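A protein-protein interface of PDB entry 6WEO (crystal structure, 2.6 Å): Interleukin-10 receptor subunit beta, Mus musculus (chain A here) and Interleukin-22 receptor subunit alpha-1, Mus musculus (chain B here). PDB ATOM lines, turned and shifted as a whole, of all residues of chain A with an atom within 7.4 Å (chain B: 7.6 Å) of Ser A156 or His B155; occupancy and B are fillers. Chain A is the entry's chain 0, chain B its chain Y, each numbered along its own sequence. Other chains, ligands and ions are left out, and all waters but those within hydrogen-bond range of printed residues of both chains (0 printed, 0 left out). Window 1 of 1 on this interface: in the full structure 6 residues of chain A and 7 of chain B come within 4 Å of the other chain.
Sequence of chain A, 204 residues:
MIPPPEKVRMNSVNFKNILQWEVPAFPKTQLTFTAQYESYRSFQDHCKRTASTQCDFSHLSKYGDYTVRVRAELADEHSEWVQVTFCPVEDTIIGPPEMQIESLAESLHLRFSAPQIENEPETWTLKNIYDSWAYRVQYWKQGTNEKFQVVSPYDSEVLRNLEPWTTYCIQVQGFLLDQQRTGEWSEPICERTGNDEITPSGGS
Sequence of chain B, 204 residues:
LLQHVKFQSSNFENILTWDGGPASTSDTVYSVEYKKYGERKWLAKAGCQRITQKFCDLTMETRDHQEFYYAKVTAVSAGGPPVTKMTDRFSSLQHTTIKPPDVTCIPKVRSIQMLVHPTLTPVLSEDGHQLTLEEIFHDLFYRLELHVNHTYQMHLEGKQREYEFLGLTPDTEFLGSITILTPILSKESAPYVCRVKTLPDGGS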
ATOM      1  N   GLN A 100      16.036   2.407 -13.822  1.00  0.00           N
ATOM      2  CA  GLN A 100      15.248   3.504 -13.270  1.00  0.00           C
ATOM      3  C   GLN A 100      15.511   3.597 -11.766  1.00  0.00           C
ATOM      4  O   GLN A 100      15.664   2.575 -11.083  1.00  0.00           O
ATOM      5  CB  GLN A 100      13.729   3.344 -13.551  1.00  0.00           C
ATOM      6  CG  GLN A 100      13.081   2.139 -12.884  1.00  0.00           C
ATOM      7  CD  GLN A 100      11.615   1.904 -13.271  1.00  0.00           C
ATOM      8  OE1 GLN A 100      11.150   0.762 -13.299  1.00  0.00           O
ATOM      9  NE2 GLN A 100      10.880   2.980 -13.541  1.00  0.00           N
ATOM     10  N   GLU A 102      14.270   5.278  -8.062  1.00  0.00           N
ATOM     11  CA  GLU A 102      13.166   5.886  -7.314  1.00  0.00           C
ATOM     12  C   GLU A 102      13.687   6.161  -5.894  1.00  0.00           C
ATOM     13  O   GLU A 102      13.517   5.334  -4.996  1.00  0.00           O
ATOM     14  CB  GLU A 102      11.921   4.966  -7.318  1.00  0.00           C
ATOM     15  CG  GLU A 102      11.284   4.634  -8.721  1.00  0.00           C
ATOM     16  CD  GLU A 102      10.532   5.778  -9.424  1.00  0.00           C
ATOM     17  OE1 GLU A 102      10.091   6.737  -8.761  1.00  0.00           O
ATOM     18  OE2 GLU A 102      10.359   5.691 -10.667  1.00  0.00           O
ATOM     19  N   HIS A 109      16.424   3.392  -4.691  1.00  0.00           N
ATOM     20  CA  HIS A 109      15.809   2.172  -5.199  1.00  0.00           C
ATOM     21  C   HIS A 109      16.104   2.026  -6.683  1.00  0.00           C
ATOM     22  O   HIS A 109      15.692   2.876  -7.486  1.00  0.00           O
ATOM     23  CB  HIS A 109      14.300   2.183  -4.930  1.00  0.00           C
ATOM     24  CG  HIS A 109      13.939   2.011  -3.483  1.00  0.00           C
ATOM     25  ND1 HIS A 109      13.343   0.869  -2.993  1.00  0.00           N
ATOM     26  CD2 HIS A 109      14.127   2.824  -2.416  1.00  0.00           C
ATOM     27  CE1 HIS A 109      13.157   0.998  -1.690  1.00  0.00           C
ATOM     28  NE2 HIS A 109      13.631   2.173  -1.315  1.00  0.00           N
ATOM     29  N   LEU A 110      16.794   0.946  -7.037  1.00  0.00           N
ATOM     30  CA  LEU A 110      17.135   0.629  -8.419  1.00  0.00           C
ATOM     31  C   LEU A 110      16.246  -0.470  -8.982  1.00  0.00           C
ATOM     32  O   LEU A 110      15.759  -1.338  -8.241  1.00  0.00           O
ATOM     33  CB  LEU A 110      18.615   0.215  -8.563  1.00  0.00           C
ATOM     34  CG  LEU A 110      19.777   1.197  -8.366  1.00  0.00           C
ATOM     35  CD1 LEU A 110      19.769   1.913  -7.049  1.00  0.00           C
ATOM     36  CD2 LEU A 110      21.127   0.490  -8.559  1.00  0.00           C
ATOM     37  N   ARG A 111      15.960  -0.368 -10.273  1.00  0.00           N
ATOM     38  CA  ARG A 111      15.296  -1.403 -11.047  1.00  0.00           C
ATOM     39  C   ARG A 111      16.017  -1.542 -12.380  1.00  0.00           C
ATOM     40  O   ARG A 111      16.299  -0.536 -13.032  1.00  0.00           O
ATOM     41  CB  ARG A 111      13.859  -1.045 -11.306  1.00  0.00           C
ATOM     42  CG  ARG A 111      13.077  -0.867 -10.078  1.00  0.00           C
ATOM     43  CD  ARG A 111      11.659  -0.483 -10.463  1.00  0.00           C
ATOM     44  NE  ARG A 111      11.005  -1.498 -11.282  1.00  0.00           N
ATOM     45  CZ  ARG A 111       9.799  -1.376 -11.836  1.00  0.00           C
ATOM     46  NH1 ARG A 111       9.057  -0.278 -11.665  1.00  0.00           N
ATOM     47  NH2 ARG A 111       9.327  -2.394 -12.543  1.00  0.00           N
ATOM     48  N   PHE A 112      16.322  -2.774 -12.775  1.00  0.00           N
ATOM     49  CA  PHE A 112      17.081  -3.073 -13.983  1.00  0.00           C
ATOM     50  C   PHE A 112      16.218  -3.775 -15.036  1.00  0.00           C
ATOM     51  O   PHE A 112      15.166  -4.365 -14.730  1.00  0.00           O
ATOM     52  CB  PHE A 112      18.305  -3.939 -13.637  1.00  0.00           C
ATOM     53  CG  PHE A 112      19.087  -3.442 -12.439  1.00  0.00           C
ATOM     54  CD1 PHE A 112      19.819  -2.258 -12.510  1.00  0.00           C
ATOM     55  CD2 PHE A 112      19.073  -4.144 -11.227  1.00  0.00           C
ATOM     56  CE1 PHE A 112      20.563  -1.796 -11.421  1.00  0.00           C
ATOM     57  CE2 PHE A 112      19.797  -3.692 -10.124  1.00  0.00           C
ATOM     58  CZ  PHE A 112      20.542  -2.508 -10.220  1.00  0.00           C
ATOM     59  N   LYS A 127      19.442 -11.829 -20.241  1.00  0.00           N
ATOM     60  CA  LYS A 127      19.265 -12.578 -18.998  1.00  0.00           C
ATOM     61  C   LYS A 127      18.536 -13.895 -19.244  1.00  0.00           C
ATOM     62  O   LYS A 127      18.743 -14.869 -18.510  1.00  0.00           O
ATOM     63  CB  LYS A 127      18.499 -11.716 -17.992  1.00  0.00           C
ATOM     64  CG  LYS A 127      18.350 -12.288 -16.619  1.00  0.00           C
ATOM     65  CD  LYS A 127      17.546 -11.342 -15.707  1.00  0.00           C
ATOM     66  CE  LYS A 127      17.350 -11.938 -14.333  1.00  0.00           C
ATOM     67  NZ  LYS A 127      16.676 -11.040 -13.345  1.00  0.00           N
ATOM     68  N   TYR A 135      24.001  -8.454 -12.233  1.00  0.00           N
ATOM     69  CA  TYR A 135      24.281  -7.034 -12.390  1.00  0.00           C
ATOM     70  C   TYR A 135      25.343  -6.561 -11.406  1.00  0.00           C
ATOM     71  O   TYR A 135      25.296  -6.892 -10.221  1.00  0.00           O
ATOM     72  CB  TYR A 135      23.016  -6.223 -12.174  1.00  0.00           C
ATOM     73  CG  TYR A 135      21.883  -6.496 -13.144  1.00  0.00           C
ATOM     74  CD1 TYR A 135      21.831  -5.891 -14.400  1.00  0.00           C
ATOM     75  CD2 TYR A 135      20.845  -7.342 -12.792  1.00  0.00           C
ATOM     76  CE1 TYR A 135      20.757  -6.119 -15.277  1.00  0.00           C
ATOM     77  CE2 TYR A 135      19.779  -7.586 -13.664  1.00  0.00           C
ATOM     78  CZ  TYR A 135      19.737  -6.976 -14.904  1.00  0.00           C
ATOM     79  OH  TYR A 135      18.669  -7.230 -15.757  1.00  0.00           O
ATOM     80  N   VAL A 137      26.607  -3.064  -9.768  1.00  0.00           N
ATOM     81  CA  VAL A 137      26.278  -1.655  -9.554  1.00  0.00           C
ATOM     82  C   VAL A 137      27.535  -0.948  -9.082  1.00  0.00           C
ATOM     83  O   VAL A 137      28.230  -1.443  -8.189  1.00  0.00           O
ATOM     84  CB  VAL A 137      25.129  -1.484  -8.543  1.00  0.00           C
ATOM     85  CG1 VAL A 137      24.905  -0.005  -8.207  1.00  0.00           C
ATOM     86  CG2 VAL A 137      23.855  -2.073  -9.096  1.00  0.00           C
ATOM     87  N   SER A 152      24.181  -7.840  -7.865  1.00  0.00           N
ATOM     88  CA  SER A 152      22.895  -8.413  -7.589  1.00  0.00           C
ATOM     89  C   SER A 152      22.439  -9.229  -8.779  1.00  0.00           C
ATOM     90  O   SER A 152      22.694  -8.845  -9.930  1.00  0.00           O
ATOM     91  CB  SER A 152      21.847  -7.356  -7.283  1.00  0.00           C
ATOM     92  OG  SER A 152      20.584  -7.977  -7.107  1.00  0.00           O
ATOM     93  N   PRO A 153      21.812 -10.378  -8.535  1.00  0.00           N
ATOM     94  CA  PRO A 153      21.268 -11.192  -9.628  1.00  0.00           C
ATOM     95  C   PRO A 153      19.824 -10.914  -9.966  1.00  0.00           C
ATOM     96  O   PRO A 153      19.311 -11.480 -10.930  1.00  0.00           O
ATOM     97  CB  PRO A 153      21.414 -12.611  -9.080  1.00  0.00           C
ATOM     98  CG  PRO A 153      21.255 -12.448  -7.594  1.00  0.00           C
ATOM     99  CD  PRO A 153      21.810 -11.094  -7.245  1.00  0.00           C
ATOM    100  N   TYR A 154      19.173 -10.042  -9.231  1.00  0.00           N
ATOM    101  CA  TYR A 154      17.759  -9.791  -9.423  1.00  0.00           C
ATOM    102  C   TYR A 154      17.609  -8.454 -10.124  1.00  0.00           C
ATOM    103  O   TYR A 154      18.567  -7.689 -10.234  1.00  0.00           O
ATOM    104  CB  TYR A 154      17.041  -9.829  -8.073  1.00  0.00           C
ATOM    105  CG  TYR A 154      17.420 -11.085  -7.315  1.00  0.00           C
ATOM    106  CD1 TYR A 154      16.901 -12.314  -7.687  1.00  0.00           C
ATOM    107  CD2 TYR A 154      18.325 -11.039  -6.262  1.00  0.00           C
ATOM    108  CE1 TYR A 154      17.264 -13.462  -7.031  1.00  0.00           C
ATOM    109  CE2 TYR A 154      18.691 -12.186  -5.590  1.00  0.00           C
ATOM    110  CZ  TYR A 154      18.161 -13.405  -5.982  1.00  0.00           C
ATOM    111  OH  TYR A 154      18.510 -14.576  -5.330  1.00  0.00           O
ATOM    112  N   ASP A 155      16.420  -8.187 -10.644  1.00  0.00           N
ATOM    113  CA  ASP A 155      16.207  -6.923 -11.350  1.00  0.00           C
ATOM    114  C   ASP A 155      15.982  -5.743 -10.427  1.00  0.00           C
ATOM    115  O   ASP A 155      15.531  -4.697 -10.892  1.00  0.00           O
ATOM    116  CB  ASP A 155      15.051  -7.021 -12.353  1.00  0.00           C
ATOM    117  CG  ASP A 155      15.404  -7.830 -13.590  1.00  0.00           C
ATOM    118  OD1 ASP A 155      16.608  -7.936 -13.920  1.00  0.00           O
ATOM    119  OD2 ASP A 155      14.469  -8.318 -14.261  1.00  0.00           O
ATOM    120  N   SER A 156      16.264  -5.857  -9.142  1.00  0.00           N
ATOM    121  CA  SER A 156      15.989  -4.754  -8.244  1.00  0.00           C
ATOM    122  C   SER A 156      17.133  -4.653  -7.244  1.00  0.00           C
ATOM    123  O   SER A 156      17.786  -5.656  -6.926  1.00  0.00           O
ATOM    124  CB  SER A 156      14.624  -4.970  -7.575  1.00  0.00           C
ATOM    125  OG  SER A 156      14.423  -4.055  -6.531  1.00  0.00           O
ATOM    126  N   GLU A 157      17.429  -3.427  -6.806  1.00  0.00           N
ATOM    127  CA  GLU A 157      18.436  -3.237  -5.763  1.00  0.00           C
ATOM    128  C   GLU A 157      18.167  -1.900  -5.082  1.00  0.00           C
ATOM    129  O   GLU A 157      17.707  -0.946  -5.724  1.00  0.00           O
ATOM    130  CB  GLU A 157      19.875  -3.259  -6.311  1.00  0.00           C
ATOM    131  CG  GLU A 157      20.673  -4.534  -6.082  1.00  0.00           C
ATOM    132  CD  GLU A 157      21.011  -4.815  -4.627  1.00  0.00           C
ATOM    133  OE1 GLU A 157      21.413  -3.867  -3.907  1.00  0.00           O
ATOM    134  OE2 GLU A 157      20.878  -5.995  -4.208  1.00  0.00           O
ATOM    135  N   VAL A 158      18.460  -1.843  -3.778  1.00  0.00           N
ATOM    136  CA  VAL A 158      18.283  -0.637  -2.968  1.00  0.00           C
ATOM    137  C   VAL A 158      19.621  -0.260  -2.350  1.00  0.00           C
ATOM    138  O   VAL A 158      20.237  -1.069  -1.646  1.00  0.00           O
ATOM    139  CB  VAL A 158      17.221  -0.807  -1.866  1.00  0.00           C
ATOM    140  CG1 VAL A 158      17.527  -2.007  -0.915  1.00  0.00           C
ATOM    141  CG2 VAL A 158      17.073   0.493  -1.075  1.00  0.00           C
ATOM    142  N   ARG B 143       9.486 -12.223  -5.923  1.00  0.00           N
ATOM    143  CA  ARG B 143       9.529 -10.858  -6.447  1.00  0.00           C
ATOM    144  C   ARG B 143       8.395 -10.106  -5.777  1.00  0.00           C
ATOM    145  O   ARG B 143       7.229 -10.504  -5.873  1.00  0.00           O
ATOM    146  CB  ARG B 143       9.383 -10.885  -7.965  1.00  0.00           C
ATOM    147  CG  ARG B 143       9.311  -9.579  -8.698  1.00  0.00           C
ATOM    148  CD  ARG B 143      10.527  -9.364  -9.580  1.00  0.00           C
ATOM    149  NE  ARG B 143      10.659 -10.353 -10.658  1.00  0.00           N
ATOM    150  CZ  ARG B 143       9.896 -10.390 -11.737  1.00  0.00           C
ATOM    151  NH1 ARG B 143       8.931  -9.499 -11.894  1.00  0.00           N
ATOM    152  NH2 ARG B 143      10.097 -11.300 -12.661  1.00  0.00           N
ATOM    153  N   LEU B 144       8.714  -9.114  -4.982  1.00  0.00           N
ATOM    154  CA  LEU B 144       7.620  -8.424  -4.337  1.00  0.00           C
ATOM    155  C   LEU B 144       7.583  -6.994  -4.823  1.00  0.00           C
ATOM    156  O   LEU B 144       8.593  -6.423  -5.254  1.00  0.00           O
ATOM    157  CB  LEU B 144       7.637  -8.499  -2.812  1.00  0.00           C
ATOM    158  CG  LEU B 144       8.654  -9.052  -1.816  1.00  0.00           C
ATOM    159  CD1 LEU B 144       8.001  -8.876  -0.476  1.00  0.00           C
ATOM    160  CD2 LEU B 144       8.995 -10.495  -1.970  1.00  0.00           C
ATOM    161  N   GLU B 145       6.366  -6.502  -4.902  1.00  0.00           N
ATOM    162  CA  GLU B 145       6.101  -5.152  -5.336  1.00  0.00           C
ATOM    163  C   GLU B 145       5.156  -4.527  -4.335  1.00  0.00           C
ATOM    164  O   GLU B 145       4.220  -5.183  -3.857  1.00  0.00           O
ATOM    165  CB  GLU B 145       5.470  -5.134  -6.739  1.00  0.00           C
ATOM    166  CG  GLU B 145       4.954  -3.793  -7.165  1.00  0.00           C
ATOM    167  CD  GLU B 145       4.218  -3.855  -8.472  1.00  0.00           C
ATOM    168  OE1 GLU B 145       4.236  -4.936  -9.110  1.00  0.00           O
ATOM    169  OE2 GLU B 145       3.664  -2.814  -8.896  1.00  0.00           O
ATOM    170  N   LEU B 146       5.411  -3.273  -4.026  1.00  0.00           N
ATOM    171  CA  LEU B 146       4.520  -2.470  -3.196  1.00  0.00           C
ATOM    172  C   LEU B 146       4.091  -1.290  -4.054  1.00  0.00           C
ATOM    173  O   LEU B 146       4.916  -0.423  -4.341  1.00  0.00           O
ATOM    174  CB  LEU B 146       5.219  -2.009  -1.912  1.00  0.00           C
ATOM    175  CG  LEU B 146       4.281  -1.551  -0.803  1.00  0.00           C
ATOM    176  CD1 LEU B 146       3.514  -2.776  -0.415  1.00  0.00           C
ATOM    177  CD2 LEU B 146       4.980  -0.952   0.407  1.00  0.00           C
ATOM    178  N   HIS B 147       2.826  -1.284  -4.490  1.00  0.00           N
ATOM    179  CA  HIS B 147       2.236  -0.289  -5.397  1.00  0.00           C
ATOM    180  C   HIS B 147       1.620   0.863  -4.591  1.00  0.00           C
ATOM    181  O   HIS B 147       0.868   0.617  -3.647  1.00  0.00           O
ATOM    182  CB  HIS B 147       1.172  -1.008  -6.240  1.00  0.00           C
ATOM    183  CG  HIS B 147       0.394  -0.149  -7.185  1.00  0.00           C
ATOM    184  ND1 HIS B 147       0.798   0.088  -8.483  1.00  0.00           N
ATOM    185  CD2 HIS B 147      -0.788   0.500  -7.035  1.00  0.00           C
ATOM    186  CE1 HIS B 147      -0.091   0.852  -9.088  1.00  0.00           C
ATOM    187  NE2 HIS B 147      -1.064   1.118  -8.232  1.00  0.00           N
ATOM    188  N   TYR B 152       4.522   5.128  -8.919  1.00  0.00           N
ATOM    189  CA  TYR B 152       5.503   4.824  -7.888  1.00  0.00           C
ATOM    190  C   TYR B 152       5.336   3.421  -7.340  1.00  0.00           C
ATOM    191  O   TYR B 152       4.274   3.057  -6.813  1.00  0.00           O
ATOM    192  CB  TYR B 152       5.434   5.854  -6.749  1.00  0.00           C
ATOM    193  CG  TYR B 152       6.574   5.703  -5.759  1.00  0.00           C
ATOM    194  CD1 TYR B 152       7.844   6.194  -6.035  1.00  0.00           C
ATOM    195  CD2 TYR B 152       6.384   5.039  -4.554  1.00  0.00           C
ATOM    196  CE1 TYR B 152       8.899   6.033  -5.119  1.00  0.00           C
ATOM    197  CE2 TYR B 152       7.420   4.874  -3.639  1.00  0.00           C
ATOM    198  CZ  TYR B 152       8.678   5.375  -3.919  1.00  0.00           C
ATOM    199  OH  TYR B 152       9.705   5.213  -3.004  1.00  0.00           O
ATOM    200  N   GLN B 153       6.404   2.643  -7.437  1.00  0.00           N
ATOM    201  CA  GLN B 153       6.404   1.296  -6.900  1.00  0.00           C
ATOM    202  C   GLN B 153       7.730   1.026  -6.216  1.00  0.00           C
ATOM    203  O   GLN B 153       8.763   1.610  -6.568  1.00  0.00           O
ATOM    204  CB  GLN B 153       6.155   0.216  -7.983  1.00  0.00           C
ATOM    205  CG  GLN B 153       4.780   0.268  -8.635  1.00  0.00           C
ATOM    206  CD  GLN B 153       4.750   1.159  -9.862  1.00  0.00           C
ATOM    207  OE1 GLN B 153       5.772   1.358 -10.545  1.00  0.00           O
ATOM    208  NE2 GLN B 153       3.588   1.742 -10.125  1.00  0.00           N
ATOM    209  N   MET B 154       7.677   0.139  -5.226  1.00  0.00           N
ATOM    210  CA  MET B 154       8.841  -0.324  -4.491  1.00  0.00           C
ATOM    211  C   MET B 154       9.038  -1.792  -4.843  1.00  0.00           C
ATOM    212  O   MET B 154       8.061  -2.532  -4.995  1.00  0.00           O
ATOM    213  CB  MET B 154       8.644  -0.171  -2.973  1.00  0.00           C
ATOM    214  CG  MET B 154       8.183   1.218  -2.494  1.00  0.00           C
ATOM    215  SD  MET B 154       9.048   1.957  -1.096  1.00  0.00           S
ATOM    216  CE  MET B 154       9.062   0.703   0.180  1.00  0.00           C
ATOM    217  N   HIS B 155      10.278  -2.211  -5.045  1.00  0.00           N
ATOM    218  CA  HIS B 155      10.486  -3.607  -5.392  1.00  0.00           C
ATOM    219  C   HIS B 155      11.510  -4.283  -4.495  1.00  0.00           C
ATOM    220  O   HIS B 155      12.596  -3.747  -4.246  1.00  0.00           O
ATOM    221  CB  HIS B 155      10.901  -3.685  -6.845  1.00  0.00           C
ATOM    222  CG  HIS B 155      10.000  -2.886  -7.716  1.00  0.00           C
ATOM    223  ND1 HIS B 155       8.886  -3.416  -8.322  1.00  0.00           N
ATOM    224  CD2 HIS B 155       9.999  -1.565  -8.007  1.00  0.00           C
ATOM    225  CE1 HIS B 155       8.255  -2.462  -8.984  1.00  0.00           C
ATOM    226  NE2 HIS B 155       8.915  -1.330  -8.814  1.00  0.00           N
ATOM    227  N   LEU B 156      11.203  -5.514  -4.118  1.00  0.00           N
ATOM    228  CA  LEU B 156      12.151  -6.390  -3.449  1.00  0.00           C
ATOM    229  C   LEU B 156      12.076  -7.775  -4.065  1.00  0.00           C
ATOM    230  O   LEU B 156      11.024  -8.198  -4.553  1.00  0.00           O
ATOM    231  CB  LEU B 156      11.921  -6.501  -1.925  1.00  0.00           C
ATOM    232  CG  LEU B 156      12.357  -5.521  -0.796  1.00  0.00           C
ATOM    233  CD1 LEU B 156      13.005  -4.260  -1.274  1.00  0.00           C
ATOM    234  CD2 LEU B 156      11.280  -5.231   0.321  1.00  0.00           C
ATOM    235  N   GLU B 157      13.225  -8.440  -4.108  1.00  0.00           N
ATOM    236  CA  GLU B 157      13.338  -9.805  -4.597  1.00  0.00           C
ATOM    237  C   GLU B 157      14.475 -10.522  -3.858  1.00  0.00           C
ATOM    238  O   GLU B 157      15.383  -9.898  -3.306  1.00  0.00           O
ATOM    239  CB  GLU B 157      13.498  -9.866  -6.141  1.00  0.00           C
ATOM    240  CG  GLU B 157      13.304  -8.539  -6.848  1.00  0.00           C
ATOM    241  CD  GLU B 157      13.579  -8.627  -8.306  1.00  0.00           C
ATOM    242  OE1 GLU B 157      13.909  -9.729  -8.741  1.00  0.00           O
ATOM    243  OE2 GLU B 157      13.502  -7.595  -9.012  1.00  0.00           O
ATOM    244  N   PHE B 165       9.295  -3.548   3.514  1.00  0.00           N
ATOM    245  CA  PHE B 165       9.388  -2.317   2.735  1.00  0.00           C
ATOM    246  C   PHE B 165       9.597  -1.191   3.734  1.00  0.00           C
ATOM    247  O   PHE B 165       8.722  -0.941   4.564  1.00  0.00           O
ATOM    248  CB  PHE B 165       8.129  -2.073   1.915  1.00  0.00           C
ATOM    249  CG  PHE B 165       7.959  -2.997   0.806  1.00  0.00           C
ATOM    250  CD1 PHE B 165       8.737  -2.876  -0.345  1.00  0.00           C
ATOM    251  CD2 PHE B 165       7.010  -4.010   0.890  1.00  0.00           C
ATOM    252  CE1 PHE B 165       8.565  -3.754  -1.421  1.00  0.00           C
ATOM    253  CE2 PHE B 165       6.813  -4.880  -0.162  1.00  0.00           C
ATOM    254  CZ  PHE B 165       7.600  -4.759  -1.325  1.00  0.00           C
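NE2 of His B155 sits at hydrogen-bond distance from NH1 of Arg A111, 3.0 Å away. The backbone NH (N) of Asp A155 sits at hydrogen-bond distance from the side-chain carboxylate (OE2) of Glu B157 (3.4 Å). The side-chain hydroxyl (OG) of Ser A156 sits at hydrogen-bond distance from the backbone carbonyl oxygen (O) of His B155 (2.9 Å). The side-chain carboxylate (OE2) of Glu B157 sits close to the backbone NH (N) of Ser A156, 3.3 Å away.
OE1 of Gln A100 sits at hydrogen-bond distance from NH1 of Arg A111 (2.9 Å). OG of Ser A156 lies close to O of Leu A110, 3.5 Å away. The backbone carbonyl oxygen (O) of Asp A155 sits at hydrogen-bond distance from the backbone NH (N) of Phe A112, 2.8 Å away. The side-chain carboxylate (OD1) of Asp A155 lies within salt-bridge range of the side-chain amino group (NZ) of Lys A127, 3.2 Å away. The side-chain hydroxyl of Tyr A135 is in hydrogen-bond range of the side-chain carboxylate of Asp A155, 2.8 Å away. The backbone NH of Tyr A154 is in hydrogen-bond range of the side-chain hydroxyl of Ser A152, 3.3 Å away.
OE1 of Glu A102 touches CD1 of Tyr B152, 3.6 Å away. OE1 of Gln B153 touches NH1 of Arg A111 (3.8 Å). CB of Tyr A154 touches OE1 of Glu B157 (3.2 Å).
Of the printed residues of chain B, Glu A102 touches Tyr B152. Of the printed residues of chain B, Arg A111 touches Gln B153 and His B155. Printed residues of chain B within 4 Å of Tyr A154: Glu B157. Of chain B, only His B155 (2.9 Å) and Glu B157 (3.2 Å) come within 4 Å of Ser A156. His B155 touches two residues of chain A.
Of the 12 printed residues of chain B, 4 touch a printed residue of chain A. Printed residues of chain B that touch a printed residue of chain A: Tyr B152, Gln B153, His B155 and Glu B157. Hydrophobic or aromatic side chains of chain B that line the printed part of chain A: Tyr B152 and His B155. Of the 16 printed residues of chain A, 5 touch a printed residue of chain B. Hydrophobic or aromatic side chains of chain A that line the printed part of chain B: Tyr A154. Along chain A the printed residues that touch a printed residue of chain B span positions 102 to 156. Among the printed residues, no Asp or Glu carboxylate lies within 4 Å of a Lys or Arg side-chain nitrogen of the other chain.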
